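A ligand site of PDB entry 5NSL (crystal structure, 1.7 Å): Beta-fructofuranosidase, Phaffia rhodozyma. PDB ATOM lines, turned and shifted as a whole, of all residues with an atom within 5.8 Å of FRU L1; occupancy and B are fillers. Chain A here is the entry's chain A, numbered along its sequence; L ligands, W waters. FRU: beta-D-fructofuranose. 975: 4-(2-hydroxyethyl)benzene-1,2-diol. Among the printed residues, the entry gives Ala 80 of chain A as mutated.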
ATOM      1  N   ASN A  79      10.711 -22.288  -7.113  1.00  0.00           N
ATOM      2  CA  ASN A  79       9.548 -23.119  -7.404  1.00  0.00           C
ATOM      3  C   ASN A  79       8.799 -23.573  -6.123  1.00  0.00           C
ATOM      4  O   ASN A  79       8.303 -22.700  -5.395  1.00  0.00           O
ATOM      5  CB  ASN A  79       9.829 -24.226  -8.471  1.00  0.00           C
ATOM      6  CG  ASN A  79      10.962 -25.184  -8.093  1.00  0.00           C
ATOM      7  OD1 ASN A  79      12.124 -24.799  -7.981  1.00  0.00           O
ATOM      8  ND2 ASN A  79      10.622 -26.468  -7.991  1.00  0.00           N
ATOM      9  N   ALA A  80       8.727 -24.871  -5.845  1.00  0.00           N
ATOM     10  CA  ALA A  80       7.828 -25.415  -4.823  1.00  0.00           C
ATOM     11  C   ALA A  80       8.060 -24.862  -3.415  1.00  0.00           C
ATOM     12  O   ALA A  80       9.204 -24.743  -2.977  1.00  0.00           O
ATOM     13  CB  ALA A  80       7.968 -26.931  -4.776  1.00  0.00           C
ATOM     14  N   GLN A  97      11.935 -23.980  -2.841  1.00  0.00           N
ATOM     15  CA  GLN A  97      12.954 -24.396  -3.795  1.00  0.00           C
ATOM     16  C   GLN A  97      13.517 -23.141  -4.457  1.00  0.00           C
ATOM     17  O   GLN A  97      12.755 -22.341  -5.004  1.00  0.00           O
ATOM     18  CB  GLN A  97      12.360 -25.340  -4.841  1.00  0.00           C
ATOM     19  CG  GLN A  97      11.926 -26.694  -4.269  1.00  0.00           C
ATOM     20  CD  GLN A  97      13.098 -27.633  -4.067  1.00  0.00           C
ATOM     21  OE1 GLN A  97      13.517 -28.311  -5.007  1.00  0.00           O
ATOM     22  NE2 GLN A  97      13.622 -27.684  -2.850  1.00  0.00           N
ATOM     23  N   TRP A 105      16.073 -23.411 -13.143  1.00  0.00           N
ATOM     24  CA  TRP A 105      16.268 -24.346 -12.033  1.00  0.00           C
ATOM     25  C   TRP A 105      17.696 -24.893 -11.993  1.00  0.00           C
ATOM     26  O   TRP A 105      18.336 -25.063 -13.025  1.00  0.00           O
ATOM     27  CB  TRP A 105      15.266 -25.487 -12.218  1.00  0.00           C
ATOM     28  CG  TRP A 105      15.193 -26.557 -11.195  1.00  0.00           C
ATOM     29  CD1 TRP A 105      14.327 -26.623 -10.140  1.00  0.00           C
ATOM     30  CD2 TRP A 105      15.954 -27.764 -11.165  1.00  0.00           C
ATOM     31  NE1 TRP A 105      14.511 -27.792  -9.448  1.00  0.00           N
ATOM     32  CE2 TRP A 105      15.514 -28.515 -10.047  1.00  0.00           C
ATOM     33  CE3 TRP A 105      16.983 -28.294 -11.968  1.00  0.00           C
ATOM     34  CZ2 TRP A 105      16.051 -29.752  -9.706  1.00  0.00           C
ATOM     35  CZ3 TRP A 105      17.530 -29.533 -11.628  1.00  0.00           C
ATOM     36  CH2 TRP A 105      17.057 -30.248 -10.506  1.00  0.00           C
ATOM     37  N   ILE A 108      19.415 -26.903  -6.535  1.00  0.00           N
ATOM     38  CA  ILE A 108      18.205 -26.432  -5.879  1.00  0.00           C
ATOM     39  C   ILE A 108      18.358 -26.538  -4.354  1.00  0.00           C
ATOM     40  O   ILE A 108      18.851 -27.532  -3.822  1.00  0.00           O
ATOM     41  CB  ILE A 108      16.929 -27.088  -6.463  1.00  0.00           C
ATOM     42  CG1 ILE A 108      15.722 -26.172  -6.270  1.00  0.00           C
ATOM     43  CG2 ILE A 108      16.699 -28.489  -5.933  1.00  0.00           C
ATOM     44  CD1 ILE A 108      15.716 -24.958  -7.184  1.00  0.00           C
ATOM     45  N   PHE A 145      15.823 -31.259  -2.754  1.00  0.00           N
ATOM     46  CA  PHE A 145      14.456 -31.217  -3.272  1.00  0.00           C
ATOM     47  C   PHE A 145      13.470 -30.956  -2.114  1.00  0.00           C
ATOM     48  O   PHE A 145      13.883 -30.711  -0.977  1.00  0.00           O
ATOM     49  CB  PHE A 145      14.127 -32.533  -4.005  1.00  0.00           C
ATOM     50  CG  PHE A 145      14.621 -32.618  -5.433  1.00  0.00           C
ATOM     51  CD1 PHE A 145      15.794 -31.978  -5.854  1.00  0.00           C
ATOM     52  CD2 PHE A 145      13.934 -33.397  -6.346  1.00  0.00           C
ATOM     53  CE1 PHE A 145      16.233 -32.101  -7.164  1.00  0.00           C
ATOM     54  CE2 PHE A 145      14.361 -33.523  -7.664  1.00  0.00           C
ATOM     55  CZ  PHE A 145      15.516 -32.873  -8.076  1.00  0.00           C
ATOM     56  N   ASP A 146      12.179 -31.014  -2.416  1.00  0.00           N
ATOM     57  CA  ASP A 146      11.096 -30.798  -1.435  1.00  0.00           C
ATOM     58  C   ASP A 146      11.244 -31.687  -0.185  1.00  0.00           C
ATOM     59  O   ASP A 146      11.755 -32.806  -0.251  1.00  0.00           O
ATOM     60  CB  ASP A 146       9.750 -31.061  -2.130  1.00  0.00           C
ATOM     61  CG  ASP A 146       8.539 -30.660  -1.305  1.00  0.00           C
ATOM     62  OD1 ASP A 146       8.640 -29.851  -0.352  1.00  0.00           O
ATOM     63  OD2 ASP A 146       7.446 -31.166  -1.645  1.00  0.00           O
ATOM     64  N   THR A 163      14.028 -34.776   0.136  1.00  0.00           N
ATOM     65  CA  THR A 163      14.621 -35.580  -0.933  1.00  0.00           C
ATOM     66  C   THR A 163      16.015 -35.065  -1.262  1.00  0.00           C
ATOM     67  O   THR A 163      16.187 -33.934  -1.737  1.00  0.00           O
ATOM     68  CB  THR A 163      13.728 -35.618  -2.187  1.00  0.00           C
ATOM     69  OG1 THR A 163      12.483 -36.246  -1.864  1.00  0.00           O
ATOM     70  CG2 THR A 163      14.406 -36.398  -3.317  1.00  0.00           C
ATOM     71  N   ARG A 220      10.201 -39.141  -4.432  1.00  0.00           N
ATOM     72  CA  ARG A 220      10.517 -37.871  -3.789  1.00  0.00           C
ATOM     73  C   ARG A 220       9.367 -37.234  -3.044  1.00  0.00           C
ATOM     74  O   ARG A 220       8.235 -37.725  -3.054  1.00  0.00           O
ATOM     75  CB  ARG A 220      11.073 -36.884  -4.830  1.00  0.00           C
ATOM     76  CG  ARG A 220      10.152 -36.590  -6.004  1.00  0.00           C
ATOM     77  CD  ARG A 220      10.688 -35.439  -6.848  1.00  0.00           C
ATOM     78  NE  ARG A 220      10.015 -35.352  -8.153  1.00  0.00           N
ATOM     79  CZ  ARG A 220      10.230 -36.157  -9.186  1.00  0.00           C
ATOM     80  NH1 ARG A 220      11.119 -37.157  -9.111  1.00  0.00           N
ATOM     81  NH2 ARG A 220       9.550 -35.987 -10.310  1.00  0.00           N
ATOM     82  N   ASP A 221       9.690 -36.122  -2.369  1.00  0.00           N
ATOM     83  CA  ASP A 221       8.735 -35.234  -1.716  1.00  0.00           C
ATOM     84  C   ASP A 221       8.092 -35.893  -0.502  1.00  0.00           C
ATOM     85  O   ASP A 221       6.872 -36.051  -0.445  1.00  0.00           O
ATOM     86  CB  ASP A 221       7.671 -34.730  -2.716  1.00  0.00           C
ATOM     87  CG  ASP A 221       8.287 -34.141  -3.974  1.00  0.00           C
ATOM     88  OD1 ASP A 221       9.479 -33.794  -3.966  1.00  0.00           O
ATOM     89  OD2 ASP A 221       7.564 -34.040  -4.985  1.00  0.00           O
ATOM     90  N   GLU A 303       3.788 -35.833  -7.729  1.00  0.00           N
ATOM     91  CA  GLU A 303       4.743 -34.973  -7.035  1.00  0.00           C
ATOM     92  C   GLU A 303       4.050 -34.210  -5.913  1.00  0.00           C
ATOM     93  O   GLU A 303       2.845 -33.950  -5.980  1.00  0.00           O
ATOM     94  CB  GLU A 303       5.374 -33.974  -8.011  1.00  0.00           C
ATOM     95  CG  GLU A 303       6.229 -34.608  -9.097  1.00  0.00           C
ATOM     96  CD  GLU A 303       6.870 -33.576  -9.998  1.00  0.00           C
ATOM     97  OE1 GLU A 303       6.126 -32.780 -10.609  1.00  0.00           O
ATOM     98  OE2 GLU A 303       8.111 -33.555 -10.106  1.00  0.00           O
ATOM     99  N   THR A 304       4.828 -33.873  -4.895  1.00  0.00           N
ATOM    100  CA  THR A 304       4.404 -33.057  -3.739  1.00  0.00           C
ATOM    101  C   THR A 304       3.069 -33.480  -3.122  1.00  0.00           C
ATOM    102  O   THR A 304       2.254 -32.621  -2.744  1.00  0.00           O
ATOM    103  CB  THR A 304       4.378 -31.541  -4.078  1.00  0.00           C
ATOM    104  OG1 THR A 304       3.253 -31.240  -4.909  1.00  0.00           O
ATOM    105  CG2 THR A 304       5.665 -31.094  -4.756  1.00  0.00           C
ATOM    106  N   GLU A 334       2.088 -35.445 -13.316  1.00  0.00           N
ATOM    107  CA  GLU A 334       2.900 -35.100 -14.475  1.00  0.00           C
ATOM    108  C   GLU A 334       2.490 -35.881 -15.709  1.00  0.00           C
ATOM    109  O   GLU A 334       2.113 -37.053 -15.622  1.00  0.00           O
ATOM    110  CB  GLU A 334       4.375 -35.411 -14.230  1.00  0.00           C
ATOM    111  CG  GLU A 334       4.942 -34.853 -12.943  1.00  0.00           C
ATOM    112  CD  GLU A 334       6.457 -34.804 -12.999  1.00  0.00           C
ATOM    113  OE1 GLU A 334       6.994 -33.748 -13.399  1.00  0.00           O
ATOM    114  OE2 GLU A 334       7.093 -35.821 -12.669  1.00  0.00           O
ATOM    115  N   HIS A 343       1.293 -30.258 -16.093  1.00  0.00           N
ATOM    116  CA  HIS A 343       1.101 -30.381 -14.641  1.00  0.00           C
ATOM    117  C   HIS A 343      -0.327 -30.087 -14.190  1.00  0.00           C
ATOM    118  O   HIS A 343      -0.875 -29.038 -14.524  1.00  0.00           O
ATOM    119  CB  HIS A 343       2.064 -29.446 -13.917  1.00  0.00           C
ATOM    120  CG  HIS A 343       3.455 -29.984 -13.762  1.00  0.00           C
ATOM    121  ND1 HIS A 343       4.552 -29.166 -13.550  1.00  0.00           N
ATOM    122  CD2 HIS A 343       3.925 -31.251 -13.794  1.00  0.00           C
ATOM    123  CE1 HIS A 343       5.630 -29.912 -13.453  1.00  0.00           C
ATOM    124  NE2 HIS A 343       5.287 -31.183 -13.591  1.00  0.00           N
ATOM    125  N   TYR A 376       1.140 -25.049  -9.204  1.00  0.00           N
ATOM    126  CA  TYR A 376       1.530 -26.431  -8.965  1.00  0.00           C
ATOM    127  C   TYR A 376       2.237 -26.507  -7.623  1.00  0.00           C
ATOM    128  O   TYR A 376       2.531 -25.477  -7.007  1.00  0.00           O
ATOM    129  CB  TYR A 376       2.476 -26.877 -10.086  1.00  0.00           C
ATOM    130  CG  TYR A 376       2.732 -28.365 -10.186  1.00  0.00           C
ATOM    131  CD1 TYR A 376       1.690 -29.256 -10.442  1.00  0.00           C
ATOM    132  CD2 TYR A 376       4.016 -28.877 -10.056  1.00  0.00           C
ATOM    133  CE1 TYR A 376       1.920 -30.621 -10.556  1.00  0.00           C
ATOM    134  CE2 TYR A 376       4.271 -30.226 -10.162  1.00  0.00           C
ATOM    135  CZ  TYR A 376       3.222 -31.101 -10.416  1.00  0.00           C
ATOM    136  OH  TYR A 376       3.458 -32.446 -10.521  1.00  0.00           O
ATOM    137  N   ALA A 377       2.494 -27.731  -7.173  1.00  0.00           N
ATOM    138  CA  ALA A 377       3.349 -27.995  -6.010  1.00  0.00           C
ATOM    139  C   ALA A 377       2.736 -27.452  -4.722  1.00  0.00           C
ATOM    140  O   ALA A 377       3.420 -26.813  -3.918  1.00  0.00           O
ATOM    141  CB  ALA A 377       4.757 -27.473  -6.232  1.00  0.00           C
ATOM    142  N   TRP A 393       2.849 -22.862  -5.819  1.00  0.00           N
ATOM    143  CA  TRP A 393       3.788 -22.076  -6.614  1.00  0.00           C
ATOM    144  C   TRP A 393       3.108 -21.648  -7.901  1.00  0.00           C
ATOM    145  O   TRP A 393       2.565 -22.496  -8.609  1.00  0.00           O
ATOM    146  CB  TRP A 393       5.026 -22.931  -6.900  1.00  0.00           C
ATOM    147  CG  TRP A 393       5.854 -22.597  -8.117  1.00  0.00           C
ATOM    148  CD1 TRP A 393       6.454 -21.406  -8.416  1.00  0.00           C
ATOM    149  CD2 TRP A 393       6.230 -23.510  -9.148  1.00  0.00           C
ATOM    150  NE1 TRP A 393       7.155 -21.514  -9.598  1.00  0.00           N
ATOM    151  CE2 TRP A 393       7.036 -22.797 -10.065  1.00  0.00           C
ATOM    152  CE3 TRP A 393       5.947 -24.862  -9.402  1.00  0.00           C
ATOM    153  CZ2 TRP A 393       7.569 -23.397 -11.217  1.00  0.00           C
ATOM    154  CZ3 TRP A 393       6.472 -25.453 -10.546  1.00  0.00           C
ATOM    155  CH2 TRP A 393       7.275 -24.713 -11.431  1.00  0.00           C
HETATM  156  C1  FRU L   1       7.564 -30.058  -7.945  1.00  0.00           C
HETATM  157  C2  FRU L   1       8.984 -30.606  -7.827  1.00  0.00           C
HETATM  158  C3  FRU L   1       9.109 -31.628  -6.713  1.00  0.00           C
HETATM  159  C4  FRU L   1      10.591 -31.584  -6.399  1.00  0.00           C
HETATM  160  C5  FRU L   1      10.954 -30.126  -6.667  1.00  0.00           C
HETATM  161  C6  FRU L   1      12.329 -29.985  -7.317  1.00  0.00           C
HETATM  162  O1  FRU L   1       7.451 -29.258  -9.120  1.00  0.00           O
HETATM  163  O2  FRU L   1       9.392 -31.203  -9.071  1.00  0.00           O
HETATM  164  O3  FRU L   1       8.650 -32.923  -7.117  1.00  0.00           O
HETATM  165  O4  FRU L   1      10.867 -31.946  -5.046  1.00  0.00           O
HETATM  166  O5  FRU L   1       9.933 -29.586  -7.499  1.00  0.00           O
HETATM  167  O6  FRU L   1      12.688 -28.603  -7.487  1.00  0.00           O
HETATM  168  CAF 975 L   2       8.953 -28.031 -13.339  1.00  0.00           C
HETATM  169  CAJ 975 L   2       9.252 -28.646 -12.115  1.00  0.00           C
HETATM  170  OAC 975 L   2       8.374 -29.464 -11.474  1.00  0.00           O
HETATM  171  CAI 975 L   2      10.494 -28.428 -11.517  1.00  0.00           C
HETATM  172  OAB 975 L   2      10.750 -29.050 -10.330  1.00  0.00           O
HETATM  173  CAD 975 L   2      11.426 -27.602 -12.137  1.00  0.00           C
HETATM  174  CAE 975 L   2      11.125 -26.996 -13.355  1.00  0.00           C
HETATM  175  CAK 975 L   2       9.878 -27.190 -13.957  1.00  0.00           C
HETATM  176  CAH 975 L   2       9.529 -26.616 -15.179  1.00  0.00           C
HETATM  177  CAG 975 L   2       9.874 -25.129 -15.209  1.00  0.00           C
HETATM  178  OAA 975 L   2       8.703 -24.349 -14.852  1.00  0.00           O
HETATM  179  CAF 975 L   3      14.371 -33.104 -12.449  1.00  0.00           C
HETATM  180  CAJ 975 L   3      15.371 -32.769 -13.367  1.00  0.00           C
HETATM  181  OAC 975 L   3      16.252 -33.691 -13.838  1.00  0.00           O
HETATM  182  CAI 975 L   3      15.502 -31.458 -13.807  1.00  0.00           C
HETATM  183  OAB 975 L   3      16.498 -31.191 -14.698  1.00  0.00           O
HETATM  184  CAD 975 L   3      14.614 -30.474 -13.358  1.00  0.00           C
HETATM  185  CAE 975 L   3      13.612 -30.815 -12.447  1.00  0.00           C
HETATM  186  CAK 975 L   3      13.470 -32.133 -11.986  1.00  0.00           C
HETATM  187  CAH 975 L   3      12.468 -32.430 -11.071  1.00  0.00           C
HETATM  188  CAG 975 L   3      11.646 -33.652 -11.472  1.00  0.00           C
HETATM  189  OAA 975 L   3      11.470 -33.618 -12.898  1.00  0.00           O
HETATM  190  O   HOH W   1       7.962 -26.986  -8.242  1.00  0.00           O
HETATM  191  O   HOH W   2       8.775 -32.066 -12.314  1.00  0.00           O
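Water W1 lies within hydrogen-bond range of O1 of FRU L1 (2.5 Å), ND2 of Asn 79 (2.7 Å) and N of Ala 80 (3.3 Å).
Water W2 lies within hydrogen-bond range of OE1 of Glu 334, OE2 of Glu 303, OAC of 975 L2, OAA of 975 L3 and O2 of FRU L1.
Phe 145 touches FRU L1.
Thr 304 touches FRU L1.
Tyr 376 touches FRU L1 (CE2 to O1, 3.5 Å).
Hydrophobic or aromatic side chains within 4 Å of FRU L1: Trp 105, Phe 145 and Tyr 376.
Of the 17 residues printed, 10 come within 4 Å of FRU L1.
The backbone NH (N) of Asp 221 lies within hydrogen-bond range of the side-chain hydroxyl (OG1) of Thr 163 (2.8 Å).
The backbone NH (N) of Asn 79 is in hydrogen-bond range of the backbone carbonyl oxygen (O) of Gln 97 (2.9 Å).
The backbone NH of Gln 97 is in hydrogen-bond range of the backbone carbonyl oxygen of Ala 80 (2.8 Å).
OE2 of Glu 303 is in salt-bridge range of NH2 of Arg 220, 2.8 Å away.
OE1 of Glu 303 sits at hydrogen-bond distance from OH of Tyr 376.
The side-chain carboxylate (OE1) of Glu 303 is in hydrogen-bond range of a ring nitrogen (NE2) of His 343 (3.5 Å).
NH2 of Arg 220 lies within salt-bridge range of OE2 of Glu 334 (3.4 Å).
O of Thr 163 lies within hydrogen-bond range of N of Phe 145 (2.9 Å).
O4 of FRU L1 lies within hydrogen-bond range of OD1 of Asp 221.
The side-chain amide oxygen of Gln 97 is in hydrogen-bond range of an oxygen (O6) of FRU L1, at 2.6 Å.
NE1 of Trp 105 lies within hydrogen-bond range of O6 of FRU L1, at 2.8 Å.
An oxygen (O2) of FRU L1 sits at hydrogen-bond distance from the side-chain carboxylate of Glu 303, at 2.9 Å.
NE of Arg 220 is in hydrogen-bond range of O3 of FRU L1.
O6 of FRU L1 is in hydrogen-bond range of ND2 of Asn 79 (3.0 Å).
O4 of FRU L1 is in hydrogen-bond range of N of Asp 146 (3.1 Å).
The side-chain amide nitrogen (ND2) of Asn 79 sits at hydrogen-bond distance from an oxygen (OAB) of 975 L2 (3.5 Å).
An oxygen (O1) of FRU L1 sits at hydrogen-bond distance from an oxygen (OAC) of 975 L2 (2.5 Å).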
